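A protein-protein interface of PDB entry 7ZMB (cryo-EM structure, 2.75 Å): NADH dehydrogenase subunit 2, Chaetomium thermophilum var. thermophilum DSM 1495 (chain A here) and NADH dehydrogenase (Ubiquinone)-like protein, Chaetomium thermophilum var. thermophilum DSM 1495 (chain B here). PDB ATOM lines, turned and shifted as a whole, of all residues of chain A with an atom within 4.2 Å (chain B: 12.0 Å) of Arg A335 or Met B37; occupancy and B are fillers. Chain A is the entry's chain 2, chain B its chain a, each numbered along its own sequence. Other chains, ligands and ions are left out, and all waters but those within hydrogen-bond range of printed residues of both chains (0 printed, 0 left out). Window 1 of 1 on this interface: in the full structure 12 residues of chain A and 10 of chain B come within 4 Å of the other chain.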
ATOM      1  N   LEU A 171     -15.316  22.127 -17.169  1.00  0.00           N
ATOM      2  CA  LEU A 171     -16.000  21.061 -16.406  1.00  0.00           C
ATOM      3  C   LEU A 171     -15.141  19.798 -16.438  1.00  0.00           C
ATOM      4  O   LEU A 171     -15.147  19.075 -15.446  1.00  0.00           O
ATOM      5  CB  LEU A 171     -17.407  20.820 -16.959  1.00  0.00           C
ATOM      6  CG  LEU A 171     -18.514  21.670 -16.357  1.00  0.00           C
ATOM      7  CD1 LEU A 171     -19.871  21.160 -16.810  1.00  0.00           C
ATOM      8  CD2 LEU A 171     -18.417  21.648 -14.847  1.00  0.00           C
ATOM      9  N   ASP A 269     -20.278  13.179 -13.717  1.00  0.00           N
ATOM     10  CA  ASP A 269     -21.156  14.244 -14.170  1.00  0.00           C
ATOM     11  C   ASP A 269     -20.403  15.378 -14.851  1.00  0.00           C
ATOM     12  O   ASP A 269     -20.984  16.069 -15.689  1.00  0.00           O
ATOM     13  CB  ASP A 269     -21.956  14.779 -12.984  1.00  0.00           C
ATOM     14  CG  ASP A 269     -23.109  15.645 -13.399  1.00  0.00           C
ATOM     15  OD1 ASP A 269     -23.637  15.447 -14.509  1.00  0.00           O
ATOM     16  OD2 ASP A 269     -23.496  16.520 -12.601  1.00  0.00           O
ATOM     17  N   ALA A 270     -19.130  15.580 -14.522  1.00  0.00           N
ATOM     18  CA  ALA A 270     -18.369  16.711 -15.040  1.00  0.00           C
ATOM     19  C   ALA A 270     -17.712  16.432 -16.387  1.00  0.00           C
ATOM     20  O   ALA A 270     -17.605  17.342 -17.214  1.00  0.00           O
ATOM     21  CB  ALA A 270     -17.304  17.132 -14.024  1.00  0.00           C
ATOM     22  N   GLN A 333     -31.746  12.630  -6.959  1.00  0.00           N
ATOM     23  CA  GLN A 333     -30.803  13.082  -8.012  1.00  0.00           C
ATOM     24  C   GLN A 333     -31.636  13.474  -9.233  1.00  0.00           C
ATOM     25  O   GLN A 333     -32.481  12.666  -9.644  1.00  0.00           O
ATOM     26  CB  GLN A 333     -29.788  11.983  -8.327  1.00  0.00           C
ATOM     27  CG  GLN A 333     -28.865  11.647  -7.165  1.00  0.00           C
ATOM     28  CD  GLN A 333     -28.062  12.825  -6.670  1.00  0.00           C
ATOM     29  OE1 GLN A 333     -27.227  13.375  -7.379  1.00  0.00           O
ATOM     30  NE2 GLN A 333     -28.293  13.211  -5.427  1.00  0.00           N
ATOM     31  N   PHE A 334     -31.464  14.695  -9.732  1.00  0.00           N
ATOM     32  CA  PHE A 334     -32.205  15.172 -10.925  1.00  0.00           C
ATOM     33  C   PHE A 334     -31.281  15.141 -12.144  1.00  0.00           C
ATOM     34  O   PHE A 334     -31.752  15.367 -13.262  1.00  0.00           O
ATOM     35  CB  PHE A 334     -32.736  16.580 -10.658  1.00  0.00           C
ATOM     36  CG  PHE A 334     -31.698  17.672 -10.632  1.00  0.00           C
ATOM     37  CD1 PHE A 334     -30.896  17.865  -9.521  1.00  0.00           C
ATOM     38  CD2 PHE A 334     -31.540  18.524 -11.711  1.00  0.00           C
ATOM     39  CE1 PHE A 334     -29.946  18.871  -9.498  1.00  0.00           C
ATOM     40  CE2 PHE A 334     -30.593  19.533 -11.685  1.00  0.00           C
ATOM     41  CZ  PHE A 334     -29.794  19.700 -10.581  1.00  0.00           C
ATOM     42  N   ARG A 335     -30.003  14.851 -11.927  1.00  0.00           N
ATOM     43  CA  ARG A 335     -29.002  14.845 -13.025  1.00  0.00           C
ATOM     44  C   ARG A 335     -28.791  13.396 -13.457  1.00  0.00           C
ATOM     45  O   ARG A 335     -28.566  12.562 -12.579  1.00  0.00           O
ATOM     46  CB  ARG A 335     -27.773  15.652 -12.594  1.00  0.00           C
ATOM     47  CG  ARG A 335     -28.056  17.136 -12.437  1.00  0.00           C
ATOM     48  CD  ARG A 335     -26.807  17.962 -12.228  1.00  0.00           C
ATOM     49  NE  ARG A 335     -25.826  17.704 -13.269  1.00  0.00           N
ATOM     50  CZ  ARG A 335     -25.756  18.341 -14.430  1.00  0.00           C
ATOM     51  NH1 ARG A 335     -24.818  18.018 -15.299  1.00  0.00           N
ATOM     52  NH2 ARG A 335     -26.619  19.296 -14.719  1.00  0.00           N
ATOM     53  N   ILE A 336     -28.875  13.114 -14.756  1.00  0.00           N
ATOM     54  CA  ILE A 336     -28.847  11.732 -15.225  1.00  0.00           C
ATOM     55  C   ILE A 336     -27.475  11.092 -14.997  1.00  0.00           C
ATOM     56  O   ILE A 336     -27.388   9.905 -14.673  1.00  0.00           O
ATOM     57  CB  ILE A 336     -29.299  11.671 -16.700  1.00  0.00           C
ATOM     58  CG1 ILE A 336     -29.538  10.229 -17.142  1.00  0.00           C
ATOM     59  CG2 ILE A 336     -28.337  12.397 -17.625  1.00  0.00           C
ATOM     60  CD1 ILE A 336     -30.824   9.631 -16.632  1.00  0.00           C
ATOM     61  N   LYS A 337     -26.384  11.845 -15.112  1.00  0.00           N
ATOM     62  CA  LYS A 337     -25.046  11.252 -14.873  1.00  0.00           C
ATOM     63  C   LYS A 337     -24.799  11.040 -13.374  1.00  0.00           C
ATOM     64  O   LYS A 337     -24.125  10.054 -13.041  1.00  0.00           O
ATOM     65  CB  LYS A 337     -23.982  11.945 -15.727  1.00  0.00           C
ATOM     66  CG  LYS A 337     -24.013  11.493 -17.182  1.00  0.00           C
ATOM     67  CD  LYS A 337     -23.459  12.479 -18.177  1.00  0.00           C
ATOM     68  CE  LYS A 337     -21.972  12.685 -18.022  1.00  0.00           C
ATOM     69  NZ  LYS A 337     -21.438  13.646 -19.010  1.00  0.00           N
ATOM     70  N   ARG A 338     -25.306  11.917 -12.502  1.00  0.00           N
ATOM     71  CA  ARG A 338     -25.221  11.668 -11.074  1.00  0.00           C
ATOM     72  C   ARG A 338     -26.086  10.484 -10.678  1.00  0.00           C
ATOM     73  O   ARG A 338     -25.742   9.745  -9.751  1.00  0.00           O
ATOM     74  CB  ARG A 338     -25.619  12.929 -10.306  1.00  0.00           C
ATOM     75  CG  ARG A 338     -24.749  14.111 -10.626  1.00  0.00           C
ATOM     76  CD  ARG A 338     -24.936  15.259  -9.671  1.00  0.00           C
ATOM     77  NE  ARG A 338     -24.813  14.860  -8.271  1.00  0.00           N
ATOM     78  CZ  ARG A 338     -23.678  14.849  -7.584  1.00  0.00           C
ATOM     79  NH1 ARG A 338     -22.543  15.199  -8.165  1.00  0.00           N
ATOM     80  NH2 ARG A 338     -23.679  14.473  -6.318  1.00  0.00           N
ATOM     81  N   LEU A 339     -27.169  10.251 -11.428  1.00  0.00           N
ATOM     82  CA  LEU A 339     -28.042   9.086 -11.136  1.00  0.00           C
ATOM     83  C   LEU A 339     -27.356   7.790 -11.558  1.00  0.00           C
ATOM     84  O   LEU A 339     -27.397   6.827 -10.782  1.00  0.00           O
ATOM     85  CB  LEU A 339     -29.404   9.229 -11.817  1.00  0.00           C
ATOM     86  CG  LEU A 339     -30.408   8.197 -11.314  1.00  0.00           C
ATOM     87  CD1 LEU A 339     -30.658   8.399  -9.832  1.00  0.00           C
ATOM     88  CD2 LEU A 339     -31.704   8.248 -12.090  1.00  0.00           C
ATOM     89  N   LEU A 404     -28.101  25.135 -18.943  1.00  0.00           N
ATOM     90  CA  LEU A 404     -27.106  24.099 -18.712  1.00  0.00           C
ATOM     91  C   LEU A 404     -25.739  24.529 -19.238  1.00  0.00           C
ATOM     92  O   LEU A 404     -25.615  25.472 -20.019  1.00  0.00           O
ATOM     93  CB  LEU A 404     -27.534  22.792 -19.373  1.00  0.00           C
ATOM     94  CG  LEU A 404     -28.669  22.056 -18.674  1.00  0.00           C
ATOM     95  CD1 LEU A 404     -29.333  21.135 -19.652  1.00  0.00           C
ATOM     96  CD2 LEU A 404     -28.162  21.301 -17.471  1.00  0.00           C
ATOM     97  N   GLN A 413     -28.224  16.087 -19.758  1.00  0.00           N
ATOM     98  CA  GLN A 413     -27.729  16.264 -18.404  1.00  0.00           C
ATOM     99  C   GLN A 413     -28.782  16.039 -17.341  1.00  0.00           C
ATOM    100  O   GLN A 413     -28.425  15.809 -16.184  1.00  0.00           O
ATOM    101  CB  GLN A 413     -27.167  17.678 -18.211  1.00  0.00           C
ATOM    102  CG  GLN A 413     -26.194  18.125 -19.260  1.00  0.00           C
ATOM    103  CD  GLN A 413     -25.268  19.180 -18.736  1.00  0.00           C
ATOM    104  OE1 GLN A 413     -25.227  19.430 -17.540  1.00  0.00           O
ATOM    105  NE2 GLN A 413     -24.523  19.813 -19.625  1.00  0.00           N
ATOM    106  N   PHE B  32     -15.298  23.525  -6.380  1.00  0.00           N
ATOM    107  CA  PHE B  32     -14.762  23.576  -7.762  1.00  0.00           C
ATOM    108  C   PHE B  32     -15.878  23.382  -8.793  1.00  0.00           C
ATOM    109  O   PHE B  32     -15.818  24.030  -9.849  1.00  0.00           O
ATOM    110  CB  PHE B  32     -13.540  22.667  -7.920  1.00  0.00           C
ATOM    111  CG  PHE B  32     -12.328  23.122  -7.149  1.00  0.00           C
ATOM    112  CD1 PHE B  32     -11.866  24.421  -7.260  1.00  0.00           C
ATOM    113  CD2 PHE B  32     -11.652  22.251  -6.312  1.00  0.00           C
ATOM    114  CE1 PHE B  32     -10.758  24.844  -6.543  1.00  0.00           C
ATOM    115  CE2 PHE B  32     -10.540  22.676  -5.600  1.00  0.00           C
ATOM    116  CZ  PHE B  32     -10.095  23.969  -5.719  1.00  0.00           C
ATOM    117  N   LEU B  33     -16.872  22.538  -8.496  1.00  0.00           N
ATOM    118  CA  LEU B  33     -17.947  22.272  -9.489  1.00  0.00           C
ATOM    119  C   LEU B  33     -19.096  23.299  -9.422  1.00  0.00           C
ATOM    120  O   LEU B  33     -19.344  23.793  -8.319  1.00  0.00           O
ATOM    121  CB  LEU B  33     -18.442  20.829  -9.408  1.00  0.00           C
ATOM    122  CG  LEU B  33     -17.697  19.806 -10.261  1.00  0.00           C
ATOM    123  CD1 LEU B  33     -18.481  18.508 -10.329  1.00  0.00           C
ATOM    124  CD2 LEU B  33     -17.449  20.334 -11.660  1.00  0.00           C
ATOM    125  N   PRO B  34     -19.810  23.652 -10.533  1.00  0.00           N
ATOM    126  CA  PRO B  34     -20.842  24.697 -10.523  1.00  0.00           C
ATOM    127  C   PRO B  34     -22.003  24.396  -9.586  1.00  0.00           C
ATOM    128  O   PRO B  34     -22.315  23.242  -9.291  1.00  0.00           O
ATOM    129  CB  PRO B  34     -21.308  24.735 -11.984  1.00  0.00           C
ATOM    130  CG  PRO B  34     -20.134  24.253 -12.738  1.00  0.00           C
ATOM    131  CD  PRO B  34     -19.578  23.157 -11.898  1.00  0.00           C
ATOM    132  N   GLU B  35     -22.652  25.470  -9.130  1.00  0.00           N
ATOM    133  CA  GLU B  35     -23.685  25.360  -8.101  1.00  0.00           C
ATOM    134  C   GLU B  35     -24.874  24.534  -8.574  1.00  0.00           C
ATOM    135  O   GLU B  35     -25.454  23.770  -7.798  1.00  0.00           O
ATOM    136  CB  GLU B  35     -24.145  26.751  -7.670  1.00  0.00           C
ATOM    137  CG  GLU B  35     -23.082  27.573  -6.961  1.00  0.00           C
ATOM    138  CD  GLU B  35     -22.700  26.990  -5.616  1.00  0.00           C
ATOM    139  OE1 GLU B  35     -23.573  26.378  -4.964  1.00  0.00           O
ATOM    140  OE2 GLU B  35     -21.530  27.148  -5.207  1.00  0.00           O
ATOM    141  N   ALA B  36     -25.259  24.681  -9.842  1.00  0.00           N
ATOM    142  CA  ALA B  36     -26.389  23.924 -10.367  1.00  0.00           C
ATOM    143  C   ALA B  36     -26.120  22.420 -10.361  1.00  0.00           C
ATOM    144  O   ALA B  36     -27.058  21.620 -10.279  1.00  0.00           O
ATOM    145  CB  ALA B  36     -26.721  24.400 -11.778  1.00  0.00           C
ATOM    146  N   MET B  37     -24.849  22.015 -10.434  1.00  0.00           N
ATOM    147  CA  MET B  37     -24.529  20.599 -10.609  1.00  0.00           C
ATOM    148  C   MET B  37     -24.411  19.861  -9.282  1.00  0.00           C
ATOM    149  O   MET B  37     -24.618  18.647  -9.229  1.00  0.00           O
ATOM    150  CB  MET B  37     -23.240  20.442 -11.414  1.00  0.00           C
ATOM    151  CG  MET B  37     -23.342  20.910 -12.853  1.00  0.00           C
ATOM    152  SD  MET B  37     -21.815  20.703 -13.762  1.00  0.00           S
ATOM    153  CE  MET B  37     -21.461  18.972 -13.487  1.00  0.00           C
ATOM    154  N   VAL B  38     -24.048  20.554  -8.204  1.00  0.00           N
ATOM    155  CA  VAL B  38     -23.828  19.897  -6.921  1.00  0.00           C
ATOM    156  C   VAL B  38     -24.560  20.593  -5.777  1.00  0.00           C
ATOM    157  O   VAL B  38     -24.477  20.148  -4.637  1.00  0.00           O
ATOM    158  CB  VAL B  38     -22.321  19.771  -6.603  1.00  0.00           C
ATOM    159  CG1 VAL B  38     -21.607  18.958  -7.668  1.00  0.00           C
ATOM    160  CG2 VAL B  38     -21.677  21.140  -6.470  1.00  0.00           C
ATOM    161  N   GLY B  39     -25.286  21.666  -6.056  1.00  0.00           N
ATOM    162  CA  GLY B  39     -25.851  22.491  -5.000  1.00  0.00           C
ATOM    163  C   GLY B  39     -27.087  21.905  -4.336  1.00  0.00           C
ATOM    164  O   GLY B  39     -27.941  21.299  -4.978  1.00  0.00           O
ATOM    165  N   ARG B  40     -27.173  22.111  -3.020  1.00  0.00           N
ATOM    166  CA  ARG B  40     -28.336  21.646  -2.272  1.00  0.00           C
ATOM    167  C   ARG B  40     -29.595  22.402  -2.672  1.00  0.00           C
ATOM    168  O   ARG B  40     -30.666  21.802  -2.815  1.00  0.00           O
ATOM    169  CB  ARG B  40     -28.099  21.800  -0.771  1.00  0.00           C
ATOM    170  CG  ARG B  40     -29.241  21.246   0.058  1.00  0.00           C
ATOM    171  CD  ARG B  40     -28.979  21.313   1.550  1.00  0.00           C
ATOM    172  NE  ARG B  40     -30.145  20.840   2.287  1.00  0.00           N
ATOM    173  CZ  ARG B  40     -30.363  19.564   2.584  1.00  0.00           C
ATOM    174  NH1 ARG B  40     -29.477  18.650   2.237  1.00  0.00           N
ATOM    175  NH2 ARG B  40     -31.453  19.205   3.246  1.00  0.00           N
ATOM    176  N   SER B  41     -29.489  23.720  -2.834  1.00  0.00           N
ATOM    177  CA  SER B  41     -30.654  24.535  -3.140  1.00  0.00           C
ATOM    178  C   SER B  41     -31.260  24.173  -4.481  1.00  0.00           C
ATOM    179  O   SER B  41     -32.453  24.405  -4.696  1.00  0.00           O
ATOM    180  CB  SER B  41     -30.279  26.017  -3.120  1.00  0.00           C
ATOM    181  OG  SER B  41     -29.285  26.302  -4.089  1.00  0.00           O
ATOM    182  N   LYS B  42     -30.465  23.609  -5.384  1.00  0.00           N
ATOM    183  CA  LYS B  42     -30.998  23.172  -6.663  1.00  0.00           C
ATOM    184  C   LYS B  42     -31.786  21.876  -6.500  1.00  0.00           C
ATOM    185  O   LYS B  42     -32.808  21.675  -7.163  1.00  0.00           O
ATOM    186  CB  LYS B  42     -29.849  23.000  -7.650  1.00  0.00           C
ATOM    187  CG  LYS B  42     -30.257  22.617  -9.038  1.00  0.00           C
ATOM    188  CD  LYS B  42     -31.004  23.762  -9.676  1.00  0.00           C
ATOM    189  CE  LYS B  42     -31.442  23.416 -11.080  1.00  0.00           C
ATOM    190  NZ  LYS B  42     -30.265  23.246 -11.972  1.00  0.00           N
ATOM    191  N   ILE B  43     -31.315  20.982  -5.627  1.00  0.00           N
ATOM    192  CA  ILE B  43     -32.107  19.822  -5.233  1.00  0.00           C
ATOM    193  C   ILE B  43     -33.371  20.272  -4.513  1.00  0.00           C
ATOM    194  O   ILE B  43     -34.440  19.671  -4.662  1.00  0.00           O
ATOM    195  CB  ILE B  43     -31.270  18.873  -4.354  1.00  0.00           C
ATOM    196  CG1 ILE B  43     -29.962  18.478  -5.050  1.00  0.00           C
ATOM    197  CG2 ILE B  43     -32.060  17.634  -3.999  1.00  0.00           C
ATOM    198  CD1 ILE B  43     -30.129  17.468  -6.157  1.00  0.00           C
ATOM    199  N   ASP B  44     -33.258  21.336  -3.714  1.00  0.00           N
ATOM    200  CA  ASP B  44     -34.408  21.856  -2.984  1.00  0.00           C
ATOM    201  C   ASP B  44     -35.485  22.354  -3.933  1.00  0.00           C
ATOM    202  O   ASP B  44     -36.679  22.238  -3.644  1.00  0.00           O
ATOM    203  CB  ASP B  44     -33.969  22.973  -2.049  1.00  0.00           C
ATOM    204  CG  ASP B  44     -33.258  22.458  -0.837  1.00  0.00           C
ATOM    205  OD1 ASP B  44     -33.399  21.257  -0.541  1.00  0.00           O
ATOM    206  OD2 ASP B  44     -32.559  23.251  -0.177  1.00  0.00           O
ATOM    207  N   GLU B  45     -35.084  22.926  -5.063  1.00  0.00           N
ATOM    208  CA  GLU B  45     -36.067  23.264  -6.080  1.00  0.00           C
ATOM    209  C   GLU B  45     -36.752  22.015  -6.617  1.00  0.00           C
ATOM    210  O   GLU B  45     -37.974  21.999  -6.795  1.00  0.00           O
ATOM    211  CB  GLU B  45     -35.405  24.046  -7.212  1.00  0.00           C
ATOM    212  CG  GLU B  45     -36.380  24.868  -8.045  1.00  0.00           C
ATOM    213  CD  GLU B  45     -35.716  25.554  -9.221  1.00  0.00           C
ATOM    214  OE1 GLU B  45     -34.599  26.086  -9.051  1.00  0.00           O
ATOM    215  OE2 GLU B  45     -36.309  25.556 -10.321  1.00  0.00           O
ATOM    216  N   LYS B  46     -35.975  20.969  -6.918  1.00  0.00           N
ATOM    217  CA  LYS B  46     -36.554  19.788  -7.616  1.00  0.00           C
ATOM    218  C   LYS B  46     -37.331  18.905  -6.648  1.00  0.00           C
ATOM    219  O   LYS B  46     -38.151  18.101  -7.114  1.00  0.00           O
ATOM    220  CB  LYS B  46     -35.429  19.000  -8.300  1.00  0.00           C
ATOM    221  CG  LYS B  46     -34.765  19.697  -9.476  1.00  0.00           C
ATOM    222  CD  LYS B  46     -35.737  20.031 -10.584  1.00  0.00           C
ATOM    223  CE  LYS B  46     -35.046  20.356 -11.888  1.00  0.00           C
ATOM    224  NZ  LYS B  46     -33.993  21.380 -11.701  1.00  0.00           N
ATOM    225  N   TYR B  47     -37.061  19.050  -5.358  1.00  0.00           N
ATOM    226  CA  TYR B  47     -37.752  18.255  -4.315  1.00  0.00           C
ATOM    227  C   TYR B  47     -38.022  19.198  -3.141  1.00  0.00           C
ATOM    228  O   TYR B  47     -37.264  19.158  -2.165  1.00  0.00           O
ATOM    229  CB  TYR B  47     -36.924  17.024  -3.935  1.00  0.00           C
ATOM    230  CG  TYR B  47     -36.502  16.149  -5.087  1.00  0.00           C
ATOM    231  CD1 TYR B  47     -35.294  16.354  -5.733  1.00  0.00           C
ATOM    232  CD2 TYR B  47     -37.304  15.111  -5.532  1.00  0.00           C
ATOM    233  CE1 TYR B  47     -34.902  15.566  -6.801  1.00  0.00           C
ATOM    234  CE2 TYR B  47     -36.923  14.306  -6.591  1.00  0.00           C
ATOM    235  CZ  TYR B  47     -35.716  14.535  -7.228  1.00  0.00           C
ATOM    236  OH  TYR B  47     -35.320  13.749  -8.270  1.00  0.00           O
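Leu A171 touches Leu B33. CD2 of Leu A171 touches CD of Pro B34, at 3.5 Å. Leu A171 touches Met B37. Asp A269 touches Met B37. Phe A334 touches Ala B36. Phe A334 touches Ile B43 (CD1 to CD1, 3.5 Å). Phe A334 touches Lys B46. Met B37 touches Arg A335 (O to CD, 3.8 Å). Met B37 touches Arg A338. NH1 of Arg A338 touches CG1 of Val B38, at 3.9 Å.
The backbone carbonyl oxygen (O) of Gln A333 sits at hydrogen-bond distance from the side-chain hydroxyl (OH) of Tyr B47 (3.3 Å).
The guanidinium group of Arg A335 lies within hydrogen-bond range of the side-chain amide oxygen of Gln A413, 2.7 Å away. The side-chain carboxylate of Asp A269 is in salt-bridge range of the guanidinium group of Arg A335, 2.7 Å away. OE1 of Gln A333 is in hydrogen-bond range of NE of Arg A338, 3.0 Å away.
Of the 16 printed residues of chain B, 9 touch a printed residue of chain A. Hydrophobic or aromatic side chains of chain A that line the printed part of chain B: Leu A171, Ala A270 and Phe A334. Among the printed residues, no Asp or Glu carboxylate lies within 4 Å of a Lys or Arg side-chain nitrogen of the other chain.
Of chain B, only Leu B33, Pro B34 and Met B37 come within 4 Å of Leu A171. Printed residues of chain B within 4 Å of Phe A334: Ala B36 (3.4 Å), Lys B42 (3.3 Å), Ile B43 (3.5 Å) and Lys B46 (3.8 Å). Arg A335 touches just one residue of chain B: Met B37 (3.8 Å). No residue of chain B comes within 4 Å of Ile A336. No residue of chain B comes within 4 Å of Lys A337. Arg A338 touches two residues of chain B. No residue of chain B comes within 4 Å of Leu A339. Printed residues of chain A within 4 Å of Ala B36: Phe A334. Arg B40 touches none of the printed residues of chain A. Ser B41 touches none of the printed residues of chain A. Of the printed residues of chain A, Lys B42 touches Phe A334. The nearest residue of chain A that does not touch Met B37 is Ala A270 (4.1 Å).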
